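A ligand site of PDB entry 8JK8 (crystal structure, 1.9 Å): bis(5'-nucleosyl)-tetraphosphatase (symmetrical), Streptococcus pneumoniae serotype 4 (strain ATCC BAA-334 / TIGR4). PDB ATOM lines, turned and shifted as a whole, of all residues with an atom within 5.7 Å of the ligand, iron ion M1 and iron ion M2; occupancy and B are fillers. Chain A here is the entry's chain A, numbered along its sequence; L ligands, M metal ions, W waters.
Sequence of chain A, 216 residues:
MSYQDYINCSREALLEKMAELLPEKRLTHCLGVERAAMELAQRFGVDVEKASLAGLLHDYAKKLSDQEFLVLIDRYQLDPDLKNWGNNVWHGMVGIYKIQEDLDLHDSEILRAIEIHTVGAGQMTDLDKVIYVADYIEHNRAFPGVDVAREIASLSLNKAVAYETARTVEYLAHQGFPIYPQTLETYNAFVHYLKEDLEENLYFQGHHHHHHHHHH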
ATOM      1  N   ARG A  26      -0.133  -6.267 -21.804  1.00  0.00           N
ATOM      2  CA  ARG A  26       0.244  -7.389 -20.953  1.00  0.00           C
ATOM      3  C   ARG A  26       1.748  -7.376 -20.635  1.00  0.00           C
ATOM      4  O   ARG A  26       2.130  -7.686 -19.501  1.00  0.00           O
ATOM      5  CB  ARG A  26      -0.223  -8.714 -21.562  1.00  0.00           C
ATOM      6  CG  ARG A  26       0.024  -9.961 -20.725  1.00  0.00           C
ATOM      7  CD  ARG A  26      -0.645  -9.884 -19.358  1.00  0.00           C
ATOM      8  NE  ARG A  26      -2.085  -9.788 -19.522  1.00  0.00           N
ATOM      9  CZ  ARG A  26      -2.967  -9.584 -18.553  1.00  0.00           C
ATOM     10  NH1 ARG A  26      -4.249  -9.534 -18.844  1.00  0.00           N
ATOM     11  NH2 ARG A  26      -2.562  -9.440 -17.292  1.00  0.00           N
ATOM     12  N   HIS A  29       2.365  -4.654 -18.173  1.00  0.00           N
ATOM     13  CA  HIS A  29       1.899  -5.211 -16.892  1.00  0.00           C
ATOM     14  C   HIS A  29       3.019  -6.032 -16.228  1.00  0.00           C
ATOM     15  O   HIS A  29       3.331  -5.816 -15.060  1.00  0.00           O
ATOM     16  CB  HIS A  29       0.617  -6.046 -17.062  1.00  0.00           C
ATOM     17  CG  HIS A  29       0.282  -6.935 -15.887  1.00  0.00           C
ATOM     18  ND1 HIS A  29      -0.039  -6.424 -14.637  1.00  0.00           N
ATOM     19  CD2 HIS A  29       0.221  -8.281 -15.756  1.00  0.00           C
ATOM     20  CE1 HIS A  29      -0.290  -7.413 -13.807  1.00  0.00           C
ATOM     21  NE2 HIS A  29      -0.136  -8.550 -14.463  1.00  0.00           N
ATOM     22  N   VAL A  33       4.920  -5.439 -12.732  1.00  0.00           N
ATOM     23  CA  VAL A  33       5.003  -6.448 -11.674  1.00  0.00           C
ATOM     24  C   VAL A  33       6.447  -6.758 -11.279  1.00  0.00           C
ATOM     25  O   VAL A  33       6.733  -6.937 -10.110  1.00  0.00           O
ATOM     26  CB  VAL A  33       4.237  -7.743 -12.043  1.00  0.00           C
ATOM     27  CG1 VAL A  33       4.374  -8.791 -10.945  1.00  0.00           C
ATOM     28  CG2 VAL A  33       2.753  -7.441 -12.221  1.00  0.00           C
ATOM     29  N   HIS A  58       5.441 -13.873 -14.474  1.00  0.00           N
ATOM     30  CA  HIS A  58       4.230 -14.487 -13.906  1.00  0.00           C
ATOM     31  C   HIS A  58       3.115 -14.704 -14.964  1.00  0.00           C
ATOM     32  O   HIS A  58       2.403 -15.720 -14.918  1.00  0.00           O
ATOM     33  CB  HIS A  58       3.730 -13.692 -12.691  1.00  0.00           C
ATOM     34  CG  HIS A  58       2.933 -12.488 -13.063  1.00  0.00           C
ATOM     35  ND1 HIS A  58       3.506 -11.364 -13.607  1.00  0.00           N
ATOM     36  CD2 HIS A  58       1.600 -12.260 -13.006  1.00  0.00           C
ATOM     37  CE1 HIS A  58       2.554 -10.482 -13.877  1.00  0.00           C
ATOM     38  NE2 HIS A  58       1.396 -11.000 -13.539  1.00  0.00           N
ATOM     39  N   ASP A  59       2.986 -13.773 -15.917  1.00  0.00           N
ATOM     40  CA  ASP A  59       1.941 -13.799 -16.947  1.00  0.00           C
ATOM     41  C   ASP A  59       2.474 -14.174 -18.324  1.00  0.00           C
ATOM     42  O   ASP A  59       1.822 -13.926 -19.341  1.00  0.00           O
ATOM     43  CB  ASP A  59       1.163 -12.472 -17.015  1.00  0.00           C
ATOM     44  CG  ASP A  59      -0.012 -12.418 -16.045  1.00  0.00           C
ATOM     45  OD1 ASP A  59      -0.383 -13.441 -15.457  1.00  0.00           O
ATOM     46  OD2 ASP A  59      -0.519 -11.318 -15.817  1.00  0.00           O
ATOM     47  N   LYS A  62       0.056 -16.118 -20.473  1.00  0.00           N
ATOM     48  CA  LYS A  62      -1.307 -15.544 -20.472  1.00  0.00           C
ATOM     49  C   LYS A  62      -2.057 -15.748 -21.800  1.00  0.00           C
ATOM     50  O   LYS A  62      -3.280 -15.884 -21.794  1.00  0.00           O
ATOM     51  CB  LYS A  62      -1.285 -14.056 -20.080  1.00  0.00           C
ATOM     52  CG  LYS A  62      -2.641 -13.385 -19.858  1.00  0.00           C
ATOM     53  CD  LYS A  62      -3.379 -13.885 -18.613  1.00  0.00           C
ATOM     54  CE  LYS A  62      -4.759 -13.261 -18.512  1.00  0.00           C
ATOM     55  NZ  LYS A  62      -5.317 -13.237 -17.127  1.00  0.00           N
ATOM     56  N   TRP A  85     -11.637 -26.193 -15.833  1.00  0.00           N
ATOM     57  CA  TRP A  85     -11.376 -24.780 -15.609  1.00  0.00           C
ATOM     58  C   TRP A  85     -10.928 -24.158 -16.920  1.00  0.00           C
ATOM     59  O   TRP A  85     -11.218 -24.707 -17.983  1.00  0.00           O
ATOM     60  CB  TRP A  85     -10.375 -24.647 -14.464  1.00  0.00           C
ATOM     61  CG  TRP A  85     -10.992 -25.257 -13.243  1.00  0.00           C
ATOM     62  CD1 TRP A  85     -10.861 -26.548 -12.817  1.00  0.00           C
ATOM     63  CD2 TRP A  85     -11.881 -24.624 -12.336  1.00  0.00           C
ATOM     64  NE1 TRP A  85     -11.610 -26.746 -11.687  1.00  0.00           N
ATOM     65  CE2 TRP A  85     -12.245 -25.582 -11.358  1.00  0.00           C
ATOM     66  CE3 TRP A  85     -12.403 -23.320 -12.230  1.00  0.00           C
ATOM     67  CZ2 TRP A  85     -13.091 -25.287 -10.289  1.00  0.00           C
ATOM     68  CZ3 TRP A  85     -13.239 -23.033 -11.167  1.00  0.00           C
ATOM     69  CH2 TRP A  85     -13.590 -24.012 -10.222  1.00  0.00           C
ATOM     70  N   ASN A  88      -7.669 -18.430 -16.707  1.00  0.00           N
ATOM     71  CA  ASN A  88      -7.494 -17.835 -15.376  1.00  0.00           C
ATOM     72  C   ASN A  88      -6.720 -18.708 -14.394  1.00  0.00           C
ATOM     73  O   ASN A  88      -5.757 -18.234 -13.805  1.00  0.00           O
ATOM     74  CB  ASN A  88      -8.839 -17.433 -14.794  1.00  0.00           C
ATOM     75  CG  ASN A  88      -9.455 -16.242 -15.519  1.00  0.00           C
ATOM     76  OD1 ASN A  88      -8.781 -15.539 -16.277  1.00  0.00           O
ATOM     77  ND2 ASN A  88     -10.739 -16.001 -15.259  1.00  0.00           N
ATOM     78  N   VAL A  89      -7.152 -19.964 -14.257  1.00  0.00           N
ATOM     79  CA  VAL A  89      -6.460 -20.965 -13.447  1.00  0.00           C
ATOM     80  C   VAL A  89      -5.195 -21.467 -14.155  1.00  0.00           C
ATOM     81  O   VAL A  89      -4.158 -21.678 -13.519  1.00  0.00           O
ATOM     82  CB  VAL A  89      -7.387 -22.167 -13.074  1.00  0.00           C
ATOM     83  CG1 VAL A  89      -6.628 -23.274 -12.358  1.00  0.00           C
ATOM     84  CG2 VAL A  89      -8.533 -21.704 -12.178  1.00  0.00           C
ATOM     85  N   HIS A  91      -3.017 -20.304 -16.639  1.00  0.00           N
ATOM     86  CA  HIS A  91      -1.846 -19.527 -17.079  1.00  0.00           C
ATOM     87  C   HIS A  91      -0.697 -19.557 -16.037  1.00  0.00           C
ATOM     88  O   HIS A  91       0.462 -19.665 -16.406  1.00  0.00           O
ATOM     89  CB  HIS A  91      -2.244 -18.122 -17.606  1.00  0.00           C
ATOM     90  CG  HIS A  91      -2.533 -17.109 -16.543  1.00  0.00           C
ATOM     91  ND1 HIS A  91      -3.798 -16.942 -16.001  1.00  0.00           N
ATOM     92  CD2 HIS A  91      -1.749 -16.175 -15.958  1.00  0.00           C
ATOM     93  CE1 HIS A  91      -3.754 -15.968 -15.099  1.00  0.00           C
ATOM     94  NE2 HIS A  91      -2.524 -15.501 -15.053  1.00  0.00           N
ATOM     95  N   HIS A 117       0.234 -17.638  -8.472  1.00  0.00           N
ATOM     96  CA  HIS A 117       0.048 -16.162  -8.487  1.00  0.00           C
ATOM     97  C   HIS A 117      -1.424 -15.704  -8.574  1.00  0.00           C
ATOM     98  O   HIS A 117      -1.748 -14.603  -8.123  1.00  0.00           O
ATOM     99  CB  HIS A 117       0.923 -15.460  -9.565  1.00  0.00           C
ATOM    100  CG  HIS A 117       0.295 -15.422 -10.931  1.00  0.00           C
ATOM    101  ND1 HIS A 117       0.592 -16.356 -11.906  1.00  0.00           N
ATOM    102  CD2 HIS A 117      -0.593 -14.556 -11.495  1.00  0.00           C
ATOM    103  CE1 HIS A 117      -0.105 -16.080 -12.997  1.00  0.00           C
ATOM    104  NE2 HIS A 117      -0.827 -14.996 -12.782  1.00  0.00           N
ATOM    105  N   THR A 118      -2.282 -16.536  -9.164  1.00  0.00           N
ATOM    106  CA  THR A 118      -3.718 -16.214  -9.404  1.00  0.00           C
ATOM    107  C   THR A 118      -4.588 -16.675  -8.225  1.00  0.00           C
ATOM    108  O   THR A 118      -5.412 -15.911  -7.718  1.00  0.00           O
ATOM    109  CB  THR A 118      -4.262 -16.847 -10.726  1.00  0.00           C
ATOM    110  OG1 THR A 118      -3.434 -16.489 -11.839  1.00  0.00           O
ATOM    111  CG2 THR A 118      -5.703 -16.393 -11.013  1.00  0.00           C
ATOM    112  N   VAL A 119      -4.377 -17.915  -7.802  1.00  0.00           N
ATOM    113  CA  VAL A 119      -5.231 -18.612  -6.826  1.00  0.00           C
ATOM    114  C   VAL A 119      -4.691 -18.663  -5.391  1.00  0.00           C
ATOM    115  O   VAL A 119      -5.442 -18.962  -4.453  1.00  0.00           O
ATOM    116  CB  VAL A 119      -5.536 -20.061  -7.279  1.00  0.00           C
ATOM    117  CG1 VAL A 119      -6.303 -20.045  -8.595  1.00  0.00           C
ATOM    118  CG2 VAL A 119      -4.259 -20.907  -7.388  1.00  0.00           C
ATOM    119  N   ASP A 135       1.324  -8.289  -8.390  1.00  0.00           N
ATOM    120  CA  ASP A 135       0.453  -8.431  -9.558  1.00  0.00           C
ATOM    121  C   ASP A 135      -0.726  -7.425  -9.483  1.00  0.00           C
ATOM    122  O   ASP A 135      -1.116  -6.767 -10.481  1.00  0.00           O
ATOM    123  CB  ASP A 135      -0.043  -9.883  -9.591  1.00  0.00           C
ATOM    124  CG  ASP A 135      -0.866 -10.197 -10.815  1.00  0.00           C
ATOM    125  OD1 ASP A 135      -0.647  -9.549 -11.866  1.00  0.00           O
ATOM    126  OD2 ASP A 135      -1.743 -11.073 -10.713  1.00  0.00           O
ATOM    127  N   ARG A 141      -1.851  -0.479 -12.811  1.00  0.00           N
ATOM    128  CA  ARG A 141      -3.224  -0.797 -12.395  1.00  0.00           C
ATOM    129  C   ARG A 141      -3.917   0.446 -11.875  1.00  0.00           C
ATOM    130  O   ARG A 141      -3.294   1.277 -11.221  1.00  0.00           O
ATOM    131  CB  ARG A 141      -3.271  -1.858 -11.297  1.00  0.00           C
ATOM    132  CG  ARG A 141      -2.496  -3.142 -11.542  1.00  0.00           C
ATOM    133  CD  ARG A 141      -3.145  -4.121 -12.511  1.00  0.00           C
ATOM    134  NE  ARG A 141      -4.521  -4.473 -12.184  1.00  0.00           N
ATOM    135  CZ  ARG A 141      -4.879  -5.669 -11.721  1.00  0.00           C
ATOM    136  NH1 ARG A 141      -6.159  -5.913 -11.491  1.00  0.00           N
ATOM    137  NH2 ARG A 141      -3.975  -6.619 -11.504  1.00  0.00           N
ATOM    138  N   GLU A 164      -6.645  -8.559  -1.124  1.00  0.00           N
ATOM    139  CA  GLU A 164      -6.753  -8.979  -2.525  1.00  0.00           C
ATOM    140  C   GLU A 164      -7.640 -10.226  -2.683  1.00  0.00           C
ATOM    141  O   GLU A 164      -8.546 -10.243  -3.540  1.00  0.00           O
ATOM    142  CB  GLU A 164      -5.383  -9.225  -3.138  1.00  0.00           C
ATOM    143  CG  GLU A 164      -5.467  -9.778  -4.556  1.00  0.00           C
ATOM    144  CD  GLU A 164      -4.138 -10.064  -5.198  1.00  0.00           C
ATOM    145  OE1 GLU A 164      -3.072  -9.717  -4.636  1.00  0.00           O
ATOM    146  OE2 GLU A 164      -4.177 -10.615  -6.325  1.00  0.00           O
ATOM    147  N   THR A 168     -11.260 -10.547  -4.652  1.00  0.00           N
ATOM    148  CA  THR A 168     -11.373 -11.497  -5.755  1.00  0.00           C
ATOM    149  C   THR A 168     -12.574 -12.416  -5.565  1.00  0.00           C
ATOM    150  O   THR A 168     -13.381 -12.576  -6.483  1.00  0.00           O
ATOM    151  CB  THR A 168     -10.060 -12.302  -5.892  1.00  0.00           C
ATOM    152  OG1 THR A 168      -9.039 -11.395  -6.318  1.00  0.00           O
ATOM    153  CG2 THR A 168     -10.179 -13.446  -6.903  1.00  0.00           C
ATOM    154  N   TYR A 171     -15.861 -10.361  -5.922  1.00  0.00           N
ATOM    155  CA  TYR A 171     -16.118 -10.042  -7.333  1.00  0.00           C
ATOM    156  C   TYR A 171     -16.545 -11.274  -8.157  1.00  0.00           C
ATOM    157  O   TYR A 171     -17.464 -11.160  -8.961  1.00  0.00           O
ATOM    158  CB  TYR A 171     -14.903  -9.351  -7.976  1.00  0.00           C
ATOM    159  CG  TYR A 171     -14.970  -9.191  -9.491  1.00  0.00           C
ATOM    160  CD1 TYR A 171     -15.618  -8.090 -10.074  1.00  0.00           C
ATOM    161  CD2 TYR A 171     -14.355 -10.121 -10.340  1.00  0.00           C
ATOM    162  CE1 TYR A 171     -15.668  -7.927 -11.454  1.00  0.00           C
ATOM    163  CE2 TYR A 171     -14.404  -9.980 -11.724  1.00  0.00           C
ATOM    164  CZ  TYR A 171     -15.052  -8.875 -12.279  1.00  0.00           C
ATOM    165  OH  TYR A 171     -15.087  -8.749 -13.654  1.00  0.00           O
ATOM    166  N   LEU A 172     -15.881 -12.421  -7.954  1.00  0.00           N
ATOM    167  CA  LEU A 172     -16.288 -13.639  -8.652  1.00  0.00           C
ATOM    168  C   LEU A 172     -17.734 -14.028  -8.324  1.00  0.00           C
ATOM    169  O   LEU A 172     -18.500 -14.386  -9.229  1.00  0.00           O
ATOM    170  CB  LEU A 172     -15.325 -14.807  -8.383  1.00  0.00           C
ATOM    171  CG  LEU A 172     -13.922 -14.650  -8.962  1.00  0.00           C
ATOM    172  CD1 LEU A 172     -13.016 -15.711  -8.379  1.00  0.00           C
ATOM    173  CD2 LEU A 172     -13.905 -14.710 -10.498  1.00  0.00           C
ATOM    174  N   PRO A 178     -17.465 -19.340 -11.475  1.00  0.00           N
ATOM    175  CA  PRO A 178     -16.950 -20.396 -10.587  1.00  0.00           C
ATOM    176  C   PRO A 178     -15.682 -19.941  -9.847  1.00  0.00           C
ATOM    177  O   PRO A 178     -14.924 -19.122 -10.367  1.00  0.00           O
ATOM    178  CB  PRO A 178     -16.595 -21.532 -11.549  1.00  0.00           C
ATOM    179  CG  PRO A 178     -17.348 -21.268 -12.808  1.00  0.00           C
ATOM    180  CD  PRO A 178     -17.529 -19.777 -12.882  1.00  0.00           C
ATOM    181  N   ILE A 179     -15.507 -20.434  -8.630  1.00  0.00           N
ATOM    182  CA  ILE A 179     -14.359 -20.063  -7.796  1.00  0.00           C
ATOM    183  C   ILE A 179     -13.491 -21.294  -7.580  1.00  0.00           C
ATOM    184  O   ILE A 179     -13.946 -22.295  -6.993  1.00  0.00           O
ATOM    185  CB  ILE A 179     -14.814 -19.448  -6.442  1.00  0.00           C
ATOM    186  CG1 ILE A 179     -15.510 -18.092  -6.674  1.00  0.00           C
ATOM    187  CG2 ILE A 179     -13.645 -19.318  -5.459  1.00  0.00           C
ATOM    188  CD1 ILE A 179     -16.394 -17.607  -5.524  1.00  0.00           C
ATOM    189  N   TYR A 180     -12.248 -21.235  -8.047  1.00  0.00           N
ATOM    190  CA  TYR A 180     -11.328 -22.347  -7.885  1.00  0.00           C
ATOM    191  C   TYR A 180     -11.176 -22.695  -6.410  1.00  0.00           C
ATOM    192  O   TYR A 180     -10.928 -21.788  -5.598  1.00  0.00           O
ATOM    193  CB  TYR A 180      -9.968 -22.020  -8.523  1.00  0.00           C
ATOM    194  CG  TYR A 180      -9.111 -23.242  -8.686  1.00  0.00           C
ATOM    195  CD1 TYR A 180      -9.516 -24.283  -9.510  1.00  0.00           C
ATOM    196  CD2 TYR A 180      -7.884 -23.349  -8.028  1.00  0.00           C
ATOM    197  CE1 TYR A 180      -8.736 -25.414  -9.670  1.00  0.00           C
ATOM    198  CE2 TYR A 180      -7.084 -24.474  -8.197  1.00  0.00           C
ATOM    199  CZ  TYR A 180      -7.522 -25.504  -9.007  1.00  0.00           C
ATOM    200  OH  TYR A 180      -6.752 -26.629  -9.175  1.00  0.00           O
ATOM    201  N   THR A 183      -8.511 -21.118  -4.315  1.00  0.00           N
ATOM    202  CA  THR A 183      -8.729 -19.701  -3.956  1.00  0.00           C
ATOM    203  C   THR A 183      -9.401 -19.593  -2.586  1.00  0.00           C
ATOM    204  O   THR A 183      -9.024 -18.715  -1.788  1.00  0.00           O
ATOM    205  CB  THR A 183      -9.476 -18.934  -5.081  1.00  0.00           C
ATOM    206  OG1 THR A 183      -8.684 -19.017  -6.264  1.00  0.00           O
ATOM    207  CG2 THR A 183      -9.725 -17.433  -4.733  1.00  0.00           C
HETATM  208  N1  LIG L   1      -9.906 -15.848 -11.174  1.00  0.00           N
HETATM  209  C1  LIG L   1      -9.306 -15.864  -9.882  1.00  0.00           C
HETATM  210  N2  LIG L   1      -9.560 -16.883  -9.020  1.00  0.00           N
HETATM  211  C2  LIG L   1     -10.386 -17.894  -9.349  1.00  0.00           C
HETATM  212  C3  LIG L   1     -11.005 -17.925 -10.613  1.00  0.00           C
HETATM  213  C4  LIG L   1     -10.742 -16.876 -11.516  1.00  0.00           C
HETATM  214  O1  LIG L   1      -8.528 -14.961  -9.507  1.00  0.00           O
HETATM  215  O2  LIG L   1     -10.601 -18.817  -8.516  1.00  0.00           O
HETATM  216  C5  LIG L   1      -9.660 -14.753 -12.162  1.00  0.00           C
HETATM  217  C6  LIG L   1      -9.588 -13.322 -11.606  1.00  0.00           C
HETATM  218  O3  LIG L   1     -10.854 -12.833 -11.153  1.00  0.00           O
HETATM  219  C7  LIG L   1      -8.929 -12.535 -12.747  1.00  0.00           C
HETATM  220  C8  LIG L   1      -8.168 -13.605 -13.523  1.00  0.00           C
HETATM  221  O4  LIG L   1      -8.420 -14.867 -12.875  1.00  0.00           O
HETATM  222  O5  LIG L   1      -9.879 -11.928 -13.635  1.00  0.00           O
HETATM  223  C9  LIG L   1      -6.679 -13.337 -13.663  1.00  0.00           C
HETATM  224  O6  LIG L   1      -6.054 -13.237 -12.380  1.00  0.00           O
HETATM  225  P1  LIG L   1      -4.485 -12.882 -12.171  1.00  0.00           P
HETATM  226  O7  LIG L   1      -3.691 -14.021 -12.745  1.00  0.00           O
HETATM  227  O8  LIG L   1      -4.304 -12.606 -10.680  1.00  0.00           O
HETATM  228  O9  LIG L   1      -4.304 -11.453 -12.969  1.00  0.00           O
HETATM  229  P2  LIG L   1      -3.903 -11.073 -14.522  1.00  0.00           P
HETATM  230  O10 LIG L   1      -3.264 -12.301 -15.179  1.00  0.00           O
HETATM  231  O11 LIG L   1      -2.910  -9.921 -14.318  1.00  0.00           O
HETATM  232  O12 LIG L   1      -5.195 -10.615 -15.186  1.00  0.00           O
HETATM  233 FE    FE M   1      -1.939 -13.772 -13.991  1.00  0.00          FE
HETATM  234 FE    FE M   2      -0.663 -10.378 -13.847  1.00  0.00          FE
HETATM  235  O   HOH W   1      -4.319  -9.143 -10.179  1.00  0.00           O
HETATM  236  O   HOH W   2      -6.143 -13.535  -8.740  1.00  0.00           O
HETATM  237  O   HOH W   3      -2.657 -12.254  -8.213  1.00  0.00           O
HETATM  238  O   HOH W   4      -3.584  -7.210 -14.754  1.00  0.00           O
HETATM  239  O   HOH W   5      -1.408 -11.972 -13.216  1.00  0.00           O
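Four residues have an atom within 4 Å of iron ion M2: His 29, His 58, Asp 59 and Asp 135.
A ring nitrogen (NE2) of His 91 sits close to the side-chain hydroxyl of Thr 118 (3.5 Å).
A ring nitrogen (NE2) of His 117 sits close to the side-chain hydroxyl (OG1) of Thr 118.
The guanidinium group (NH2) of Arg 26 lies close to the side-chain carboxylate (OD2) of Asp 59 (3.1 Å).
The side-chain hydroxyl (OG1) of Thr 168 lies within hydrogen-bond range of the backbone carbonyl oxygen (O) of Glu 164 (3.0 Å).
A ring nitrogen (ND1) of His 91 sits at hydrogen-bond distance from the backbone carbonyl oxygen (O) of Asn 88, 3.2 Å away.
The backbone carbonyl oxygen (O) of Asp 135 is in hydrogen-bond range of the guanidinium group (NH2) of Arg 141.
Iron ion M1 is bound by water W5, NE2 of His 117, NE2 of His 91, OD1 of Asp 59, O7 of the ligand and O10 of the ligand.
Residues that only touch iron ion M1: Thr 118 (3.8 Å).
Five residues have an atom within 4 Å of iron ion M1: His 58, Asp 59, His 91, His 117 and Thr 118.
The nearest printed residue that does not touch iron ion M1 is Asp 135 (4.3 Å).
Residues that only touch the ligand: Thr 168, Leu 172 and Ile 179.
Hydrophobic or aromatic side chains within 4 Å of the ligand: His 29, His 91, His 117, Leu 172 and Tyr 180.
Within 4 Å of the ligand: Arg 26, His 29, Asp 59, Lys 62, Asn 88, His 91, His 117, Thr 118, Asp 135, Thr 168, Leu 172, Ile 179, Tyr 180 and Thr 183.
The nearest printed residue that does not touch the ligand is Pro 178 (4.1 Å).
Water W5 binds iron ion M2 (1.9 Å).
NE2 of His 29 binds iron ion M2, at 2.0 Å.
OD1 of Asp 135 binds iron ion M2, 2.1 Å away.
Iron ion M2 is bound by NE2 of His 58 (2.2 Å).
The side-chain carboxylate (OD2) of Asp 59 is bound to iron ion M2, at 2.2 Å.
An oxygen (O11) of the ligand binds iron ion M2, 2.3 Å away.
Iron ion M2 has six donor atoms within binding distance.
Water W5 bridges OD2 of Asp 135 and O9 of the ligand.
Water W2 bridges O of Thr 118 (2.7 Å) and O8 of the ligand (2.8 Å).
Water W1 lies within hydrogen-bond range of NH2 of Arg 141 (2.9 Å), OD2 of Asp 135 (3.3 Å) and O8 of the ligand (3.5 Å).
The backbone NH (N) of Tyr 180 sits at hydrogen-bond distance from an oxygen (O2) of the ligand (3.0 Å).
An oxygen (O12) of the ligand is in salt-bridge range of the guanidinium group of Arg 26.
An oxygen (O7) of the ligand sits close to the side-chain hydroxyl (OG1) of Thr 118, at 2.6 Å.
The side-chain amino group (NZ) of Lys 62 is in salt-bridge range of an oxygen (O12) of the ligand (3.3 Å).
The side-chain amide oxygen (OD1) of Asn 88 lies close to an oxygen (O4) of the ligand (3.5 Å).
The side-chain hydroxyl (OG1) of Thr 183 sits at hydrogen-bond distance from an oxygen (O2) of the ligand.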
